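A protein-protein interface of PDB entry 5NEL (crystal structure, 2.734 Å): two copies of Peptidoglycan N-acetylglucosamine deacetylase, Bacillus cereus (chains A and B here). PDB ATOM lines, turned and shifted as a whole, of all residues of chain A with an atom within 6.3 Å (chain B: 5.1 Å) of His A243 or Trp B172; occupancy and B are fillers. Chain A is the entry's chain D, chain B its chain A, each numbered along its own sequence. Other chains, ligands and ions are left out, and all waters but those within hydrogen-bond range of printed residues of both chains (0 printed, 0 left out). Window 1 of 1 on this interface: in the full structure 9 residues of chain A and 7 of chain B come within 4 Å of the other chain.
The indole nitrogen (NE1) of Trp B172 is in hydrogen-bond range of a ring nitrogen (ND1) of His A243 (3.1 Å).
The backbone carbonyl oxygen (O) of Trp B172 lies within hydrogen-bond range of the side-chain amide nitrogen (ND2) of Asn A245.
The guanidinium group (NH2) of Arg B173 lies within hydrogen-bond range of the backbone carbonyl oxygen (O) of Pro A238, at 3.1 Å.
The backbone NH (N) of Asn B175 lies close to the side-chain amide nitrogen (ND2) of Asn A245.
The backbone carbonyl oxygen of Arg B173 sits close to the side-chain amide nitrogen of Asn A245.
The side-chain amide oxygen (OD1) of Asn B175 lies close to the backbone carbonyl oxygen (O) of Asp B171, 2.9 Å away.
ND2 of Asn B175 lies within hydrogen-bond range of NE2 of His B207 (3.1 Å).
The side-chain amide oxygen (OD1) of Asn A240 lies within hydrogen-bond range of the backbone NH (N) of His A243, 3.2 Å away.
CE1 of Tyr B141 touches CE of Met A144, at 3.3 Å.
O of Pro A238 touches CH2 of Trp B172, at 3.5 Å.
CG2 of Val A239 touches NH2 of Arg B173, at 3.6 Å.
CD1 of Tyr B141 touches O of Phe A241, at 3.8 Å.
Tyr B174 touches Asn A245 (N to ND2, 3.9 Å).
Of chain B, only Trp B172 (2.9 Å) comes within 4 Å of His A243.
Of the printed residues of chain B, Pro A238 touches Trp B172 and Arg B173.
Of the printed residues of chain A, Tyr B174 touches Asn A245.
Printed residues of chain A within 4 Å of Tyr B141: Met A144 and Phe A241.
Of the printed residues of chain B, Asn A245 touches Trp B172, Arg B173, Tyr B174 and Asn B175.
The nearest residue of chain B that does not touch His A243 is Tyr B141 (4.8 Å).
The nearest residue of chain A that does not touch Trp B172 is Asn A240 (4.1 Å).
The nearest printed residue of chain B that does not touch Asn A245 is Asp B171 (5.9 Å).
Of the 10 printed residues of chain A, 6 touch a printed residue of chain B.
Hydrophobic or aromatic side chains of chain A that line the printed part of chain B: Met A144, Pro A238, Val A239 and His A243.
Hydrophobic or aromatic side chains of chain B within 4 Å of the printed part of chain A: Tyr B141 and Trp B172.
Among the printed residues, no Asp or Glu carboxylate lies within 4 Å of a Lys or Arg side-chain nitrogen of the other chain.
No position is printed for both chains.
Of the 10 pairs that touch across the chains among the printed residues, none has its exchanged pair printed and touching as well.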
ATOM      1  N   MET A 144     -26.027   2.237  16.801  1.00  0.00           N
ATOM      2  CA  MET A 144     -25.076   1.186  17.142  1.00  0.00           C
ATOM      3  C   MET A 144     -25.524  -0.171  16.628  1.00  0.00           C
ATOM      4  O   MET A 144     -26.565  -0.669  17.055  1.00  0.00           O
ATOM      5  CB  MET A 144     -24.903   1.125  18.655  1.00  0.00           C
ATOM      6  CG  MET A 144     -23.935   0.070  19.141  1.00  0.00           C
ATOM      7  SD  MET A 144     -22.205   0.588  19.011  1.00  0.00           S
ATOM      8  CE  MET A 144     -22.194   2.029  20.053  1.00  0.00           C
ATOM      9  N   PRO A 238     -26.552  15.969  23.448  1.00  0.00           N
ATOM     10  CA  PRO A 238     -26.310  14.670  22.798  1.00  0.00           C
ATOM     11  C   PRO A 238     -26.924  13.481  23.516  1.00  0.00           C
ATOM     12  O   PRO A 238     -26.863  13.383  24.740  1.00  0.00           O
ATOM     13  CB  PRO A 238     -24.785  14.552  22.805  1.00  0.00           C
ATOM     14  CG  PRO A 238     -24.355  15.421  23.913  1.00  0.00           C
ATOM     15  CD  PRO A 238     -25.302  16.573  23.937  1.00  0.00           C
ATOM     16  N   VAL A 239     -27.535  12.597  22.735  1.00  0.00           N
ATOM     17  CA  VAL A 239     -28.019  11.311  23.231  1.00  0.00           C
ATOM     18  C   VAL A 239     -27.746  10.251  22.165  1.00  0.00           C
ATOM     19  O   VAL A 239     -28.609   9.965  21.322  1.00  0.00           O
ATOM     20  CB  VAL A 239     -29.528  11.323  23.569  1.00  0.00           C
ATOM     21  CG1 VAL A 239     -30.019   9.921  23.916  1.00  0.00           C
ATOM     22  CG2 VAL A 239     -29.815  12.247  24.723  1.00  0.00           C
ATOM     23  N   ASN A 240     -26.540   9.686  22.174  1.00  0.00           N
ATOM     24  CA  ASN A 240     -26.270   8.584  21.262  1.00  0.00           C
ATOM     25  C   ASN A 240     -25.393   7.494  21.848  1.00  0.00           C
ATOM     26  O   ASN A 240     -24.616   7.699  22.793  1.00  0.00           O
ATOM     27  CB  ASN A 240     -25.661   9.094  19.953  1.00  0.00           C
ATOM     28  CG  ASN A 240     -24.299   9.720  20.133  1.00  0.00           C
ATOM     29  OD1 ASN A 240     -23.282   9.092  19.853  1.00  0.00           O
ATOM     30  ND2 ASN A 240     -24.271  10.975  20.561  1.00  0.00           N
ATOM     31  N   PHE A 241     -25.559   6.314  21.277  1.00  0.00           N
ATOM     32  CA  PHE A 241     -24.881   5.131  21.762  1.00  0.00           C
ATOM     33  C   PHE A 241     -23.353   5.203  21.616  1.00  0.00           C
ATOM     34  O   PHE A 241     -22.626   4.492  22.318  1.00  0.00           O
ATOM     35  CB  PHE A 241     -25.437   3.919  21.032  1.00  0.00           C
ATOM     36  CG  PHE A 241     -26.893   3.692  21.285  1.00  0.00           C
ATOM     37  CD1 PHE A 241     -27.460   4.057  22.501  1.00  0.00           C
ATOM     38  CD2 PHE A 241     -27.700   3.127  20.307  1.00  0.00           C
ATOM     39  CE1 PHE A 241     -28.810   3.849  22.753  1.00  0.00           C
ATOM     40  CE2 PHE A 241     -29.074   2.929  20.530  1.00  0.00           C
ATOM     41  CZ  PHE A 241     -29.631   3.290  21.756  1.00  0.00           C
ATOM     42  N   TRP A 242     -22.871   6.072  20.726  1.00  0.00           N
ATOM     43  CA  TRP A 242     -21.438   6.202  20.481  1.00  0.00           C
ATOM     44  C   TRP A 242     -20.821   7.267  21.367  1.00  0.00           C
ATOM     45  O   TRP A 242     -19.634   7.568  21.233  1.00  0.00           O
ATOM     46  CB  TRP A 242     -21.150   6.554  19.018  1.00  0.00           C
ATOM     47  CG  TRP A 242     -21.490   5.490  18.042  1.00  0.00           C
ATOM     48  CD1 TRP A 242     -22.711   5.242  17.489  1.00  0.00           C
ATOM     49  CD2 TRP A 242     -20.603   4.515  17.497  1.00  0.00           C
ATOM     50  NE1 TRP A 242     -22.638   4.177  16.628  1.00  0.00           N
ATOM     51  CE2 TRP A 242     -21.350   3.713  16.611  1.00  0.00           C
ATOM     52  CE3 TRP A 242     -19.247   4.240  17.668  1.00  0.00           C
ATOM     53  CZ2 TRP A 242     -20.793   2.655  15.913  1.00  0.00           C
ATOM     54  CZ3 TRP A 242     -18.691   3.200  16.957  1.00  0.00           C
ATOM     55  CH2 TRP A 242     -19.460   2.414  16.097  1.00  0.00           C
ATOM     56  N   HIS A 243     -21.626   7.860  22.247  1.00  0.00           N
ATOM     57  CA  HIS A 243     -21.142   8.934  23.115  1.00  0.00           C
ATOM     58  C   HIS A 243     -20.459  10.057  22.345  1.00  0.00           C
ATOM     59  O   HIS A 243     -19.628  10.754  22.901  1.00  0.00           O
ATOM     60  CB  HIS A 243     -20.139   8.417  24.151  1.00  0.00           C
ATOM     61  CG  HIS A 243     -20.630   7.258  24.954  1.00  0.00           C
ATOM     62  ND1 HIS A 243     -21.790   7.304  25.697  1.00  0.00           N
ATOM     63  CD2 HIS A 243     -20.106   6.022  25.147  1.00  0.00           C
ATOM     64  CE1 HIS A 243     -21.966   6.142  26.302  1.00  0.00           C
ATOM     65  NE2 HIS A 243     -20.959   5.348  25.984  1.00  0.00           N
ATOM     66  N   ASP A 244     -20.767  10.200  21.064  1.00  0.00           N
ATOM     67  CA  ASP A 244     -20.198  11.273  20.252  1.00  0.00           C
ATOM     68  C   ASP A 244     -21.043  12.533  20.427  1.00  0.00           C
ATOM     69  O   ASP A 244     -22.221  12.573  20.052  1.00  0.00           O
ATOM     70  CB  ASP A 244     -20.135  10.852  18.778  1.00  0.00           C
ATOM     71  CG  ASP A 244     -19.424  11.866  17.902  1.00  0.00           C
ATOM     72  OD1 ASP A 244     -19.286  13.035  18.328  1.00  0.00           O
ATOM     73  OD2 ASP A 244     -19.011  11.492  16.778  1.00  0.00           O
ATOM     74  N   ASN A 245     -20.449  13.567  21.001  1.00  0.00           N
ATOM     75  CA  ASN A 245     -21.222  14.764  21.283  1.00  0.00           C
ATOM     76  C   ASN A 245     -21.062  15.798  20.170  1.00  0.00           C
ATOM     77  O   ASN A 245     -21.210  16.995  20.396  1.00  0.00           O
ATOM     78  CB  ASN A 245     -20.835  15.359  22.640  1.00  0.00           C
ATOM     79  CG  ASN A 245     -19.381  15.768  22.705  1.00  0.00           C
ATOM     80  OD1 ASN A 245     -18.666  15.778  21.696  1.00  0.00           O
ATOM     81  ND2 ASN A 245     -18.932  16.113  23.899  1.00  0.00           N
ATOM     82  N   ARG A 246     -20.744  15.322  18.974  1.00  0.00           N
ATOM     83  CA  ARG A 246     -20.809  16.155  17.788  1.00  0.00           C
ATOM     84  C   ARG A 246     -22.219  16.066  17.189  1.00  0.00           C
ATOM     85  O   ARG A 246     -22.601  16.872  16.339  1.00  0.00           O
ATOM     86  CB  ARG A 246     -19.734  15.738  16.781  1.00  0.00           C
ATOM     87  CG  ARG A 246     -18.298  15.858  17.335  1.00  0.00           C
ATOM     88  CD  ARG A 246     -17.258  15.409  16.324  1.00  0.00           C
ATOM     89  NE  ARG A 246     -17.639  14.127  15.737  1.00  0.00           N
ATOM     90  CZ  ARG A 246     -17.255  13.706  14.535  1.00  0.00           C
ATOM     91  NH1 ARG A 246     -16.464  14.468  13.787  1.00  0.00           N
ATOM     92  NH2 ARG A 246     -17.670  12.527  14.079  1.00  0.00           N
ATOM     93  N   TYR B 141     -20.452  -0.606  26.498  1.00  0.00           N
ATOM     94  CA  TYR B 141     -21.800  -0.133  26.150  1.00  0.00           C
ATOM     95  C   TYR B 141     -22.886  -0.679  27.059  1.00  0.00           C
ATOM     96  O   TYR B 141     -24.074  -0.526  26.754  1.00  0.00           O
ATOM     97  CB  TYR B 141     -22.150  -0.462  24.696  1.00  0.00           C
ATOM     98  CG  TYR B 141     -21.109  -0.031  23.677  1.00  0.00           C
ATOM     99  CD1 TYR B 141     -20.886   1.311  23.401  1.00  0.00           C
ATOM    100  CD2 TYR B 141     -20.356  -0.974  22.978  1.00  0.00           C
ATOM    101  CE1 TYR B 141     -19.931   1.704  22.471  1.00  0.00           C
ATOM    102  CE2 TYR B 141     -19.401  -0.592  22.046  1.00  0.00           C
ATOM    103  CZ  TYR B 141     -19.199   0.751  21.787  1.00  0.00           C
ATOM    104  OH  TYR B 141     -18.261   1.136  20.849  1.00  0.00           O
ATOM    105  N   ASP B 168     -24.674   7.181  35.908  1.00  0.00           N
ATOM    106  CA  ASP B 168     -23.905   7.570  34.735  1.00  0.00           C
ATOM    107  C   ASP B 168     -23.496   9.027  34.863  1.00  0.00           C
ATOM    108  O   ASP B 168     -24.348   9.914  34.938  1.00  0.00           O
ATOM    109  CB  ASP B 168     -24.704   7.339  33.448  1.00  0.00           C
ATOM    110  CG  ASP B 168     -23.852   7.476  32.177  1.00  0.00           C
ATOM    111  OD1 ASP B 168     -22.811   8.178  32.185  1.00  0.00           O
ATOM    112  OD2 ASP B 168     -24.224   6.866  31.153  1.00  0.00           O
ATOM    113  N   LEU B 170     -22.111  10.880  32.643  1.00  0.00           N
ATOM    114  CA  LEU B 170     -22.345  11.615  31.398  1.00  0.00           C
ATOM    115  C   LEU B 170     -21.122  12.444  30.990  1.00  0.00           C
ATOM    116  O   LEU B 170     -21.238  13.392  30.212  1.00  0.00           O
ATOM    117  CB  LEU B 170     -23.592  12.514  31.507  1.00  0.00           C
ATOM    118  CG  LEU B 170     -24.997  11.927  31.295  1.00  0.00           C
ATOM    119  CD1 LEU B 170     -25.241  10.623  32.046  1.00  0.00           C
ATOM    120  CD2 LEU B 170     -26.053  12.956  31.665  1.00  0.00           C
ATOM    121  N   ASP B 171     -19.942  12.061  31.472  1.00  0.00           N
ATOM    122  CA  ASP B 171     -18.739  12.849  31.217  1.00  0.00           C
ATOM    123  C   ASP B 171     -18.423  13.039  29.717  1.00  0.00           C
ATOM    124  O   ASP B 171     -17.775  14.023  29.331  1.00  0.00           O
ATOM    125  CB  ASP B 171     -17.529  12.230  31.946  1.00  0.00           C
ATOM    126  CG  ASP B 171     -17.347  10.737  31.666  1.00  0.00           C
ATOM    127  OD1 ASP B 171     -18.291   9.957  31.904  1.00  0.00           O
ATOM    128  OD2 ASP B 171     -16.246  10.342  31.217  1.00  0.00           O
ATOM    129  N   TRP B 172     -18.888  12.118  28.877  1.00  0.00           N
ATOM    130  CA  TRP B 172     -18.590  12.179  27.449  1.00  0.00           C
ATOM    131  C   TRP B 172     -19.306  13.344  26.748  1.00  0.00           C
ATOM    132  O   TRP B 172     -18.904  13.765  25.657  1.00  0.00           O
ATOM    133  CB  TRP B 172     -18.958  10.860  26.772  1.00  0.00           C
ATOM    134  CG  TRP B 172     -20.426  10.530  26.865  1.00  0.00           C
ATOM    135  CD1 TRP B 172     -21.032   9.742  27.798  1.00  0.00           C
ATOM    136  CD2 TRP B 172     -21.459  10.989  25.997  1.00  0.00           C
ATOM    137  NE1 TRP B 172     -22.381   9.680  27.563  1.00  0.00           N
ATOM    138  CE2 TRP B 172     -22.673  10.441  26.463  1.00  0.00           C
ATOM    139  CE3 TRP B 172     -21.481  11.822  24.877  1.00  0.00           C
ATOM    140  CZ2 TRP B 172     -23.906  10.695  25.840  1.00  0.00           C
ATOM    141  CZ3 TRP B 172     -22.700  12.059  24.252  1.00  0.00           C
ATOM    142  CH2 TRP B 172     -23.899  11.501  24.742  1.00  0.00           C
ATOM    143  N   ARG B 173     -20.380  13.843  27.357  1.00  0.00           N
ATOM    144  CA  ARG B 173     -21.097  14.974  26.791  1.00  0.00           C
ATOM    145  C   ARG B 173     -20.176  16.163  26.704  1.00  0.00           C
ATOM    146  O   ARG B 173     -20.176  16.871  25.706  1.00  0.00           O
ATOM    147  CB  ARG B 173     -22.326  15.336  27.627  1.00  0.00           C
ATOM    148  CG  ARG B 173     -23.335  14.243  27.640  1.00  0.00           C
ATOM    149  CD  ARG B 173     -24.650  14.653  28.255  1.00  0.00           C
ATOM    150  NE  ARG B 173     -25.660  13.688  27.828  1.00  0.00           N
ATOM    151  CZ  ARG B 173     -26.957  13.751  28.105  1.00  0.00           C
ATOM    152  NH1 ARG B 173     -27.436  14.751  28.837  1.00  0.00           N
ATOM    153  NH2 ARG B 173     -27.770  12.802  27.647  1.00  0.00           N
ATOM    154  N   TYR B 174     -19.373  16.358  27.744  1.00  0.00           N
ATOM    155  CA  TYR B 174     -18.589  17.574  27.894  1.00  0.00           C
ATOM    156  C   TYR B 174     -17.154  17.444  27.381  1.00  0.00           C
ATOM    157  O   TYR B 174     -16.257  18.156  27.838  1.00  0.00           O
ATOM    158  CB  TYR B 174     -18.577  17.985  29.364  1.00  0.00           C
ATOM    159  CG  TYR B 174     -19.889  17.750  30.070  1.00  0.00           C
ATOM    160  CD1 TYR B 174     -20.904  18.689  30.006  1.00  0.00           C
ATOM    161  CD2 TYR B 174     -20.111  16.599  30.798  1.00  0.00           C
ATOM    162  CE1 TYR B 174     -22.111  18.488  30.650  1.00  0.00           C
ATOM    163  CE2 TYR B 174     -21.316  16.385  31.453  1.00  0.00           C
ATOM    164  CZ  TYR B 174     -22.318  17.335  31.372  1.00  0.00           C
ATOM    165  OH  TYR B 174     -23.527  17.143  32.015  1.00  0.00           O
ATOM    166  N   ASN B 175     -16.944  16.549  26.418  1.00  0.00           N
ATOM    167  CA  ASN B 175     -15.600  16.289  25.899  1.00  0.00           C
ATOM    168  C   ASN B 175     -15.060  17.404  25.014  1.00  0.00           C
ATOM    169  O   ASN B 175     -15.819  18.153  24.397  1.00  0.00           O
ATOM    170  CB  ASN B 175     -15.567  14.966  25.123  1.00  0.00           C
ATOM    171  CG  ASN B 175     -15.563  13.742  26.039  1.00  0.00           C
ATOM    172  OD1 ASN B 175     -15.694  13.850  27.273  1.00  0.00           O
ATOM    173  ND2 ASN B 175     -15.425  12.570  25.435  1.00  0.00           N
ATOM    174  N   HIS B 207     -10.542  10.632  30.003  1.00  0.00           N
ATOM    175  CA  HIS B 207     -11.099  11.967  29.790  1.00  0.00           C
ATOM    176  C   HIS B 207     -10.652  12.912  30.885  1.00  0.00           C
ATOM    177  O   HIS B 207     -10.777  12.592  32.065  1.00  0.00           O
ATOM    178  CB  HIS B 207     -12.630  11.936  29.750  1.00  0.00           C
ATOM    179  CG  HIS B 207     -13.179  11.261  28.538  1.00  0.00           C
ATOM    180  ND1 HIS B 207     -12.503  11.231  27.337  1.00  0.00           N
ATOM    181  CD2 HIS B 207     -14.323  10.561  28.353  1.00  0.00           C
ATOM    182  CE1 HIS B 207     -13.212  10.548  26.456  1.00  0.00           C
ATOM    183  NE2 HIS B 207     -14.319  10.130  27.048  1.00  0.00           N
